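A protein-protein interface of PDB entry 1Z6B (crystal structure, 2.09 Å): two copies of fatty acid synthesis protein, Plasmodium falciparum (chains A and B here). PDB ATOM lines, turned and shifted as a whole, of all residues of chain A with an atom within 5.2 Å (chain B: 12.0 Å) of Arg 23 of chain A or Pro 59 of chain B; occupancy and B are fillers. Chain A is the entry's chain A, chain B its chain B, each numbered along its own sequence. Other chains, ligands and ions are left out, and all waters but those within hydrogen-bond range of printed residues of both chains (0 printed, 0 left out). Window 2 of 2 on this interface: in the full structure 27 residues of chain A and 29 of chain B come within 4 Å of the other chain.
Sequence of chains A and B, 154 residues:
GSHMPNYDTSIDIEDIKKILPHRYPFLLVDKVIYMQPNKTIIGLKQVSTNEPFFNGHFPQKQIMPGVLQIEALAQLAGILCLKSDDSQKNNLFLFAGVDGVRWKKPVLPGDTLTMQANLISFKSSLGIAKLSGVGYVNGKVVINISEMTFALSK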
ATOM      1  N   LYS A  17      17.649  10.963   6.138  1.00  0.00           N
ATOM      2  CA  LYS A  17      17.468  11.932   5.055  1.00  0.00           C
ATOM      3  C   LYS A  17      16.144  11.789   4.317  1.00  0.00           C
ATOM      4  O   LYS A  17      15.606  12.774   3.796  1.00  0.00           O
ATOM      5  CB  LYS A  17      18.677  11.903   4.104  1.00  0.00           C
ATOM      6  CG  LYS A  17      19.882  12.635   4.712  1.00  0.00           C
ATOM      7  CD  LYS A  17      21.202  12.400   3.982  1.00  0.00           C
ATOM      8  CE  LYS A  17      21.229  13.107   2.648  1.00  0.00           C
ATOM      9  NZ  LYS A  17      22.612  13.314   2.147  1.00  0.00           N
ATOM     10  N   LYS A  18      15.595  10.578   4.298  1.00  0.00           N
ATOM     11  CA  LYS A  18      14.307  10.329   3.689  1.00  0.00           C
ATOM     12  C   LYS A  18      13.193  10.808   4.596  1.00  0.00           C
ATOM     13  O   LYS A  18      12.082  11.042   4.136  1.00  0.00           O
ATOM     14  CB  LYS A  18      14.127   8.824   3.407  1.00  0.00           C
ATOM     15  CG  LYS A  18      15.116   8.254   2.402  1.00  0.00           C
ATOM     16  CD  LYS A  18      14.931   6.757   2.235  1.00  0.00           C
ATOM     17  CE  LYS A  18      16.104   6.109   1.479  1.00  0.00           C
ATOM     18  NZ  LYS A  18      15.844   4.636   1.251  1.00  0.00           N
ATOM     19  N   LEU A  20      13.788  13.462   7.197  1.00  0.00           N
ATOM     20  CA  LEU A  20      13.970  14.908   7.409  1.00  0.00           C
ATOM     21  C   LEU A  20      14.314  15.667   6.133  1.00  0.00           C
ATOM     22  O   LEU A  20      15.011  15.153   5.256  1.00  0.00           O
ATOM     23  CB  LEU A  20      15.092  15.195   8.420  1.00  0.00           C
ATOM     24  CG  LEU A  20      14.793  14.784   9.857  1.00  0.00           C
ATOM     25  CD1 LEU A  20      16.013  15.022  10.734  1.00  0.00           C
ATOM     26  CD2 LEU A  20      13.554  15.511  10.388  1.00  0.00           C
ATOM     27  N   PRO A  21      13.841  16.902   6.054  1.00  0.00           N
ATOM     28  CA  PRO A  21      14.194  17.793   4.948  1.00  0.00           C
ATOM     29  C   PRO A  21      15.592  18.429   5.079  1.00  0.00           C
ATOM     30  O   PRO A  21      16.144  18.901   4.083  1.00  0.00           O
ATOM     31  CB  PRO A  21      13.096  18.853   5.010  1.00  0.00           C
ATOM     32  CG  PRO A  21      12.753  18.956   6.479  1.00  0.00           C
ATOM     33  CD  PRO A  21      12.926  17.547   7.015  1.00  0.00           C
ATOM     34  N   HIS A  22      16.159  18.396   6.286  1.00  0.00           N
ATOM     35  CA  HIS A  22      17.408  19.089   6.609  1.00  0.00           C
ATOM     36  C   HIS A  22      18.574  18.465   5.894  1.00  0.00           C
ATOM     37  O   HIS A  22      18.648  17.242   5.790  1.00  0.00           O
ATOM     38  CB  HIS A  22      17.725  18.981   8.110  1.00  0.00           C
ATOM     39  CG  HIS A  22      16.647  19.492   9.008  1.00  0.00           C
ATOM     40  ND1 HIS A  22      15.499  18.774   9.284  1.00  0.00           N
ATOM     41  CD2 HIS A  22      16.561  20.632   9.726  1.00  0.00           C
ATOM     42  CE1 HIS A  22      14.738  19.472  10.108  1.00  0.00           C
ATOM     43  NE2 HIS A  22      15.358  20.603  10.392  1.00  0.00           N
ATOM     44  N   ARG A  23      19.526  19.299   5.481  1.00  0.00           N
ATOM     45  CA  ARG A  23      20.672  18.866   4.708  1.00  0.00           C
ATOM     46  C   ARG A  23      21.890  19.676   5.150  1.00  0.00           C
ATOM     47  O   ARG A  23      21.743  20.587   5.955  1.00  0.00           O
ATOM     48  CB  ARG A  23      20.387  19.086   3.227  1.00  0.00           C
ATOM     49  CG  ARG A  23      19.366  18.139   2.635  1.00  0.00           C
ATOM     50  CD  ARG A  23      19.742  16.665   2.736  1.00  0.00           C
ATOM     51  NE  ARG A  23      18.717  15.869   2.070  1.00  0.00           N
ATOM     52  CZ  ARG A  23      17.670  15.314   2.669  1.00  0.00           C
ATOM     53  NH1 ARG A  23      17.466  15.410   3.967  1.00  0.00           N
ATOM     54  NH2 ARG A  23      16.800  14.638   1.950  1.00  0.00           N
ATOM     55  N   TYR A  24      23.077  19.330   4.654  1.00  0.00           N
ATOM     56  CA  TYR A  24      24.291  20.068   4.992  1.00  0.00           C
ATOM     57  C   TYR A  24      24.101  21.568   4.695  1.00  0.00           C
ATOM     58  O   TYR A  24      23.585  21.888   3.638  1.00  0.00           O
ATOM     59  CB  TYR A  24      25.467  19.540   4.191  1.00  0.00           C
ATOM     60  CG  TYR A  24      26.805  20.202   4.486  1.00  0.00           C
ATOM     61  CD1 TYR A  24      27.562  19.785   5.556  1.00  0.00           C
ATOM     62  CD2 TYR A  24      27.328  21.208   3.671  1.00  0.00           C
ATOM     63  CE1 TYR A  24      28.788  20.325   5.841  1.00  0.00           C
ATOM     64  CE2 TYR A  24      28.588  21.781   3.960  1.00  0.00           C
ATOM     65  CZ  TYR A  24      29.301  21.325   5.074  1.00  0.00           C
ATOM     66  OH  TYR A  24      30.540  21.783   5.455  1.00  0.00           O
ATOM     67  N   PRO A  25      24.468  22.466   5.616  1.00  0.00           N
ATOM     68  CA  PRO A  25      25.265  22.164   6.802  1.00  0.00           C
ATOM     69  C   PRO A  25      24.367  22.258   8.035  1.00  0.00           C
ATOM     70  O   PRO A  25      24.762  22.771   9.072  1.00  0.00           O
ATOM     71  CB  PRO A  25      26.319  23.311   6.811  1.00  0.00           C
ATOM     72  CG  PRO A  25      25.548  24.451   6.260  1.00  0.00           C
ATOM     73  CD  PRO A  25      24.653  23.870   5.204  1.00  0.00           C
ATOM     74  N   PHE A  26      23.148  21.767   7.933  1.00  0.00           N
ATOM     75  CA  PHE A  26      22.236  21.906   9.045  1.00  0.00           C
ATOM     76  C   PHE A  26      21.451  20.639   9.377  1.00  0.00           C
ATOM     77  O   PHE A  26      20.334  20.722   9.904  1.00  0.00           O
ATOM     78  CB  PHE A  26      21.293  23.105   8.796  1.00  0.00           C
ATOM     79  CG  PHE A  26      21.119  23.966  10.002  1.00  0.00           C
ATOM     80  CD1 PHE A  26      22.112  24.880  10.368  1.00  0.00           C
ATOM     81  CD2 PHE A  26      20.008  23.856  10.785  1.00  0.00           C
ATOM     82  CE1 PHE A  26      21.981  25.661  11.501  1.00  0.00           C
ATOM     83  CE2 PHE A  26      19.862  24.647  11.906  1.00  0.00           C
ATOM     84  CZ  PHE A  26      20.862  25.544  12.271  1.00  0.00           C
ATOM     85  N   LEU A  27      22.057  19.493   9.091  1.00  0.00           N
ATOM     86  CA  LEU A  27      21.562  18.198   9.550  1.00  0.00           C
ATOM     87  C   LEU A  27      22.487  17.671  10.666  1.00  0.00           C
ATOM     88  O   LEU A  27      23.673  17.371  10.462  1.00  0.00           O
ATOM     89  CB  LEU A  27      21.434  17.212   8.374  1.00  0.00           C
ATOM     90  CG  LEU A  27      20.992  15.768   8.680  1.00  0.00           C
ATOM     91  CD1 LEU A  27      19.547  15.754   9.071  1.00  0.00           C
ATOM     92  CD2 LEU A  27      21.207  14.936   7.481  1.00  0.00           C
ATOM     93  N   THR B  49      20.090  34.991   1.008  1.00  0.00           N
ATOM     94  CA  THR B  49      20.201  33.648   0.488  1.00  0.00           C
ATOM     95  C   THR B  49      21.668  33.157   0.483  1.00  0.00           C
ATOM     96  O   THR B  49      21.935  31.971   0.628  1.00  0.00           O
ATOM     97  CB  THR B  49      19.520  33.548  -0.921  1.00  0.00           C
ATOM     98  OG1 THR B  49      19.529  32.186  -1.374  1.00  0.00           O
ATOM     99  CG2 THR B  49      20.263  34.368  -2.013  1.00  0.00           C
ATOM    100  N   GLU B  51      23.986  32.902   2.581  1.00  0.00           N
ATOM    101  CA  GLU B  51      24.514  32.404   3.872  1.00  0.00           C
ATOM    102  C   GLU B  51      24.553  30.887   3.880  1.00  0.00           C
ATOM    103  O   GLU B  51      23.627  30.270   3.372  1.00  0.00           O
ATOM    104  CB  GLU B  51      23.589  32.852   4.996  1.00  0.00           C
ATOM    105  CG  GLU B  51      23.549  34.367   5.161  1.00  0.00           C
ATOM    106  CD  GLU B  51      22.839  34.839   6.422  1.00  0.00           C
ATOM    107  OE1 GLU B  51      23.370  34.649   7.539  1.00  0.00           O
ATOM    108  OE2 GLU B  51      21.791  35.490   6.266  1.00  0.00           O
ATOM    109  N   PRO B  52      25.608  30.288   4.441  1.00  0.00           N
ATOM    110  CA  PRO B  52      25.846  28.843   4.291  1.00  0.00           C
ATOM    111  C   PRO B  52      24.755  27.925   4.826  1.00  0.00           C
ATOM    112  O   PRO B  52      24.608  26.833   4.313  1.00  0.00           O
ATOM    113  CB  PRO B  52      27.191  28.604   5.000  1.00  0.00           C
ATOM    114  CG  PRO B  52      27.324  29.797   5.964  1.00  0.00           C
ATOM    115  CD  PRO B  52      26.657  30.932   5.248  1.00  0.00           C
ATOM    116  N   PHE B  53      23.970  28.368   5.798  1.00  0.00           N
ATOM    117  CA  PHE B  53      23.021  27.483   6.452  1.00  0.00           C
ATOM    118  C   PHE B  53      21.741  27.286   5.620  1.00  0.00           C
ATOM    119  O   PHE B  53      21.024  26.321   5.837  1.00  0.00           O
ATOM    120  CB  PHE B  53      22.702  27.977   7.856  1.00  0.00           C
ATOM    121  CG  PHE B  53      22.111  29.363   7.904  1.00  0.00           C
ATOM    122  CD1 PHE B  53      20.795  29.594   7.512  1.00  0.00           C
ATOM    123  CD2 PHE B  53      22.880  30.433   8.301  1.00  0.00           C
ATOM    124  CE1 PHE B  53      20.258  30.857   7.550  1.00  0.00           C
ATOM    125  CE2 PHE B  53      22.346  31.715   8.322  1.00  0.00           C
ATOM    126  CZ  PHE B  53      21.024  31.922   7.953  1.00  0.00           C
ATOM    127  N   PHE B  54      21.446  28.206   4.695  1.00  0.00           N
ATOM    128  CA  PHE B  54      20.226  28.114   3.874  1.00  0.00           C
ATOM    129  C   PHE B  54      20.145  26.925   2.913  1.00  0.00           C
ATOM    130  O   PHE B  54      19.049  26.442   2.641  1.00  0.00           O
ATOM    131  CB  PHE B  54      19.976  29.397   3.085  1.00  0.00           C
ATOM    132  CG  PHE B  54      19.212  30.446   3.852  1.00  0.00           C
ATOM    133  CD1 PHE B  54      17.953  30.168   4.391  1.00  0.00           C
ATOM    134  CD2 PHE B  54      19.752  31.732   4.020  1.00  0.00           C
ATOM    135  CE1 PHE B  54      17.248  31.142   5.079  1.00  0.00           C
ATOM    136  CE2 PHE B  54      19.064  32.707   4.717  1.00  0.00           C
ATOM    137  CZ  PHE B  54      17.802  32.428   5.250  1.00  0.00           C
ATOM    138  N   ASN B  55      21.279  26.457   2.390  1.00  0.00           N
ATOM    139  CA  ASN B  55      21.258  25.214   1.590  1.00  0.00           C
ATOM    140  C   ASN B  55      20.671  24.017   2.402  1.00  0.00           C
ATOM    141  O   ASN B  55      20.163  23.073   1.840  1.00  0.00           O
ATOM    142  CB  ASN B  55      22.663  24.861   1.045  1.00  0.00           C
ATOM    143  CG  ASN B  55      22.904  25.343  -0.403  1.00  0.00           C
ATOM    144  OD1 ASN B  55      22.023  25.894  -1.009  1.00  0.00           O
ATOM    145  ND2 ASN B  55      24.109  25.097  -0.951  1.00  0.00           N
ATOM    146  N   GLY B  56      20.754  24.078   3.722  1.00  0.00           N
ATOM    147  CA  GLY B  56      20.413  22.955   4.581  1.00  0.00           C
ATOM    148  C   GLY B  56      19.080  23.095   5.276  1.00  0.00           C
ATOM    149  O   GLY B  56      18.604  22.130   5.882  1.00  0.00           O
ATOM    150  N   HIS B  57      18.466  24.284   5.170  1.00  0.00           N
ATOM    151  CA  HIS B  57      17.297  24.654   5.962  1.00  0.00           C
ATOM    152  C   HIS B  57      16.404  25.625   5.230  1.00  0.00           C
ATOM    153  O   HIS B  57      16.317  26.776   5.602  1.00  0.00           O
ATOM    154  CB  HIS B  57      17.757  25.267   7.275  1.00  0.00           C
ATOM    155  CG  HIS B  57      16.733  25.244   8.367  1.00  0.00           C
ATOM    156  ND1 HIS B  57      15.737  26.187   8.481  1.00  0.00           N
ATOM    157  CD2 HIS B  57      16.585  24.416   9.432  1.00  0.00           C
ATOM    158  CE1 HIS B  57      14.999  25.926   9.545  1.00  0.00           C
ATOM    159  NE2 HIS B  57      15.505  24.868  10.151  1.00  0.00           N
ATOM    160  N   PHE B  58      15.695  25.189   4.191  1.00  0.00           N
ATOM    161  CA  PHE B  58      15.707  23.820   3.665  1.00  0.00           C
ATOM    162  C   PHE B  58      15.928  23.893   2.173  1.00  0.00           C
ATOM    163  O   PHE B  58      15.670  24.931   1.570  1.00  0.00           O
ATOM    164  CB  PHE B  58      14.362  23.140   3.952  1.00  0.00           C
ATOM    165  CG  PHE B  58      14.016  23.126   5.397  1.00  0.00           C
ATOM    166  CD1 PHE B  58      14.556  22.163   6.233  1.00  0.00           C
ATOM    167  CD2 PHE B  58      13.188  24.089   5.931  1.00  0.00           C
ATOM    168  CE1 PHE B  58      14.259  22.146   7.568  1.00  0.00           C
ATOM    169  CE2 PHE B  58      12.883  24.081   7.274  1.00  0.00           C
ATOM    170  CZ  PHE B  58      13.412  23.117   8.092  1.00  0.00           C
ATOM    171  N   PRO B  59      16.390  22.800   1.571  1.00  0.00           N
ATOM    172  CA  PRO B  59      16.550  22.780   0.125  1.00  0.00           C
ATOM    173  C   PRO B  59      15.365  23.397  -0.596  1.00  0.00           C
ATOM    174  O   PRO B  59      15.567  24.264  -1.426  1.00  0.00           O
ATOM    175  CB  PRO B  59      16.739  21.288  -0.196  1.00  0.00           C
ATOM    176  CG  PRO B  59      17.463  20.746   1.019  1.00  0.00           C
ATOM    177  CD  PRO B  59      16.840  21.536   2.189  1.00  0.00           C
ATOM    178  N   GLN B  60      14.138  23.012  -0.251  1.00  0.00           N
ATOM    179  CA  GLN B  60      12.977  23.502  -1.003  1.00  0.00           C
ATOM    180  C   GLN B  60      12.252  24.711  -0.417  1.00  0.00           C
ATOM    181  O   GLN B  60      11.313  25.209  -1.014  1.00  0.00           O
ATOM    182  CB  GLN B  60      12.014  22.350  -1.300  1.00  0.00           C
ATOM    183  CG  GLN B  60      12.463  21.515  -2.501  1.00  0.00           C
ATOM    184  CD  GLN B  60      12.875  20.104  -2.133  1.00  0.00           C
ATOM    185  OE1 GLN B  60      12.007  19.224  -1.968  1.00  0.00           O
ATOM    186  NE2 GLN B  60      14.193  19.863  -2.040  1.00  0.00           N
ATOM    187  N   LYS B  61      12.704  25.208   0.724  1.00  0.00           N
ATOM    188  CA  LYS B  61      12.110  26.399   1.327  1.00  0.00           C
ATOM    189  C   LYS B  61      13.118  27.021   2.275  1.00  0.00           C
ATOM    190  O   LYS B  61      13.449  26.434   3.314  1.00  0.00           O
ATOM    191  CB  LYS B  61      10.828  26.038   2.074  1.00  0.00           C
ATOM    192  CG  LYS B  61       9.956  27.230   2.422  1.00  0.00           C
ATOM    193  CD  LYS B  61       8.704  26.749   3.116  1.00  0.00           C
ATOM    194  CE  LYS B  61       7.737  27.880   3.434  1.00  0.00           C
ATOM    195  NZ  LYS B  61       6.463  27.316   3.984  1.00  0.00           N
ATOM    196  N   GLN B  62      13.653  28.184   1.895  1.00  0.00           N
ATOM    197  CA  GLN B  62      14.711  28.824   2.699  1.00  0.00           C
ATOM    198  C   GLN B  62      14.095  29.597   3.864  1.00  0.00           C
ATOM    199  O   GLN B  62      13.411  30.580   3.651  1.00  0.00           O
ATOM    200  CB  GLN B  62      15.578  29.730   1.827  1.00  0.00           C
ATOM    201  CG  GLN B  62      16.230  29.001   0.679  1.00  0.00           C
ATOM    202  CD  GLN B  62      17.485  29.656   0.192  1.00  0.00           C
ATOM    203  OE1 GLN B  62      17.638  30.860   0.331  1.00  0.00           O
ATOM    204  NE2 GLN B  62      18.405  28.860  -0.370  1.00  0.00           N
ATOM    205  N   ILE B  63      14.375  29.139   5.087  1.00  0.00           N
ATOM    206  CA  ILE B  63      13.825  29.692   6.314  1.00  0.00           C
ATOM    207  C   ILE B  63      14.942  29.788   7.338  1.00  0.00           C
ATOM    208  O   ILE B  63      15.631  28.807   7.596  1.00  0.00           O
ATOM    209  CB  ILE B  63      12.695  28.765   6.850  1.00  0.00           C
ATOM    210  CG1 ILE B  63      11.456  28.864   5.959  1.00  0.00           C
ATOM    211  CG2 ILE B  63      12.323  29.127   8.321  1.00  0.00           C
ATOM    212  CD1 ILE B  63      10.358  27.917   6.343  1.00  0.00           C
ATOM    213  N   MET B  64      15.172  30.970   7.905  1.00  0.00           N
ATOM    214  CA  MET B  64      16.266  31.106   8.868  1.00  0.00           C
ATOM    215  C   MET B  64      15.961  30.259  10.090  1.00  0.00           C
ATOM    216  O   MET B  64      14.917  30.441  10.716  1.00  0.00           O
ATOM    217  CB  MET B  64      16.463  32.553   9.301  1.00  0.00           C
ATOM    218  CG  MET B  64      17.692  32.751  10.229  1.00  0.00           C
ATOM    219  SD  MET B  64      17.905  34.460  10.785  1.00  0.00           S
ATOM    220  CE  MET B  64      19.339  34.232  11.852  1.00  0.00           C
ATOM    221  N   PRO B  65      16.838  29.326  10.449  1.00  0.00           N
ATOM    222  CA  PRO B  65      16.555  28.477  11.603  1.00  0.00           C
ATOM    223  C   PRO B  65      16.253  29.341  12.809  1.00  0.00           C
ATOM    224  O   PRO B  65      16.988  30.293  13.068  1.00  0.00           O
ATOM    225  CB  PRO B  65      17.853  27.716  11.818  1.00  0.00           C
ATOM    226  CG  PRO B  65      18.493  27.717  10.522  1.00  0.00           C
ATOM    227  CD  PRO B  65      18.110  28.978   9.818  1.00  0.00           C
ATOM    228  N   VAL B  67      16.823  28.599  15.845  1.00  0.00           N
ATOM    229  CA  VAL B  67      17.895  28.533  16.828  1.00  0.00           C
ATOM    230  C   VAL B  67      18.999  29.570  16.543  1.00  0.00           C
ATOM    231  O   VAL B  67      19.691  29.995  17.470  1.00  0.00           O
ATOM    232  CB  VAL B  67      18.489  27.132  16.968  1.00  0.00           C
ATOM    233  CG1 VAL B  67      17.379  26.114  17.330  1.00  0.00           C
ATOM    234  CG2 VAL B  67      19.296  26.744  15.718  1.00  0.00           C
ATOM    235  N   LEU B  68      19.131  29.977  15.278  1.00  0.00           N
ATOM    236  CA  LEU B  68      20.115  30.992  14.893  1.00  0.00           C
ATOM    237  C   LEU B  68      19.613  32.389  15.206  1.00  0.00           C
ATOM    238  O   LEU B  68      20.402  33.310  15.327  1.00  0.00           O
ATOM    239  CB  LEU B  68      20.444  30.898  13.407  1.00  0.00           C
ATOM    240  CG  LEU B  68      21.214  29.644  12.997  1.00  0.00           C
ATOM    241  CD1 LEU B  68      21.665  29.779  11.584  1.00  0.00           C
ATOM    242  CD2 LEU B  68      22.388  29.350  13.917  1.00  0.00           C
ATOM    243  N   LEU B 108      12.948  35.177   6.408  1.00  0.00           N
ATOM    244  CA  LEU B 108      13.294  34.721   5.062  1.00  0.00           C
ATOM    245  C   LEU B 108      14.421  35.576   4.405  1.00  0.00           C
ATOM    246  O   LEU B 108      14.611  36.745   4.770  1.00  0.00           O
ATOM    247  CB  LEU B 108      12.037  34.776   4.209  1.00  0.00           C
ATOM    248  CG  LEU B 108      10.801  34.245   4.925  1.00  0.00           C
ATOM    249  CD1 LEU B 108       9.623  34.515   4.031  1.00  0.00           C
ATOM    250  CD2 LEU B 108      10.867  32.764   5.329  1.00  0.00           C
ATOM    251  N   PRO B 109      15.163  34.998   3.453  1.00  0.00           N
ATOM    252  CA  PRO B 109      16.092  35.783   2.635  1.00  0.00           C
ATOM    253  C   PRO B 109      15.472  37.098   2.227  1.00  0.00           C
ATOM    254  O   PRO B 109      14.289  37.145   1.821  1.00  0.00           O
ATOM    255  CB  PRO B 109      16.324  34.898   1.418  1.00  0.00           C
ATOM    256  CG  PRO B 109      16.161  33.457   1.955  1.00  0.00           C
ATOM    257  CD  PRO B 109      15.210  33.559   3.110  1.00  0.00           C
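The backbone NH (N) of Arg 23 of chain A is in hydrogen-bond range of the backbone carbonyl oxygen (O) of Gly 56 of chain B (3.0 Å).
NH2 of Arg 23 of chain A lies within hydrogen-bond range of O of Lys 17 of chain A, at 2.9 Å. The backbone carbonyl oxygen of Leu 20 of chain A is in hydrogen-bond range of the guanidinium group of Arg 23 of chain A (2.8 Å). The backbone carbonyl oxygen (O) of Ile 63 of chain B lies within hydrogen-bond range of a ring nitrogen (ND1) of His 57 of chain B (2.8 Å).
CD1 of Phe 58 of chain B touches CG of Pro 21 of chain A, at 3.7 Å. CA of His 22 of chain A touches O of Gly 56 of chain B (3.3 Å). His 22 of chain A touches His 57 of chain B. Pro 59 of chain B touches Arg 23 of chain A. O of Tyr 24 of chain A touches C of Asn 55 of chain B, 3.8 Å away. O of Pro 52 of chain B touches CD of Pro 25 of chain A, at 3.1 Å. Pro 25 of chain A touches Phe 53 of chain B. Phe 26 of chain A touches His 57 of chain B. Phe 26 of chain A touches Pro 65 of chain B (CE2 to CG, 3.6 Å). Phe 26 of chain A touches Val 67 of chain B (CZ to CG2, 3.97 Å).
No residue of chain B comes within 4 Å of Lys 17 of chain A. No residue of chain B comes within 4 Å of Leu 20 of chain A. Of chain B, only Phe 58 (3.7 Å) and Pro 59 (3.3 Å) come within 4 Å of Pro 21 of chain A. His 22 of chain A touches just these residues of chain B: Gly 56 (3.3 Å), His 57 (3.8 Å) and Phe 58 (3.4 Å). Arg 23 of chain A touches just these residues of chain B: Gly 56 and Pro 59. Of chain B, only Pro 52 and Phe 53 come within 4 Å of Pro 25 of chain A. No residue of chain B comes within 4 Å of Leu 27 of chain A. Of the printed residues of chain A, Phe 53 of chain B touches Pro 25 (3.95 Å). Phe 54 of chain B touches none of the printed residues of chain A. Of the printed residues of chain A, Gly 56 of chain B touches His 22 (3.3 Å), Arg 23 (3.0 Å) and Tyr 24 (3.5 Å). Of the printed residues of chain A, Pro 59 of chain B touches Pro 21 (3.3 Å) and Arg 23 (3.6 Å). The nearest printed residue of chain B that does not touch Phe 26 of chain A is Phe 53 of chain B (4.03 Å).
Printed residues of chain A that touch a printed residue of chain B: Pro 21, His 22, Arg 23, Tyr 24, Pro 25 and Phe 26. Hydrophobic or aromatic side chains of chain A within 4 Å of the printed part of chain B: Pro 21, His 22, Pro 25 and Phe 26. Of the 20 printed residues of chain B, 9 touch a printed residue of chain A. Hydrophobic or aromatic side chains of chain B within 4 Å of the printed part of chain A: His 57, Phe 58, Pro 59, Pro 65 and Val 67. Along chain B the printed residues that touch a printed residue of chain A span positions 52 to 67.
No position is printed for both chains.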
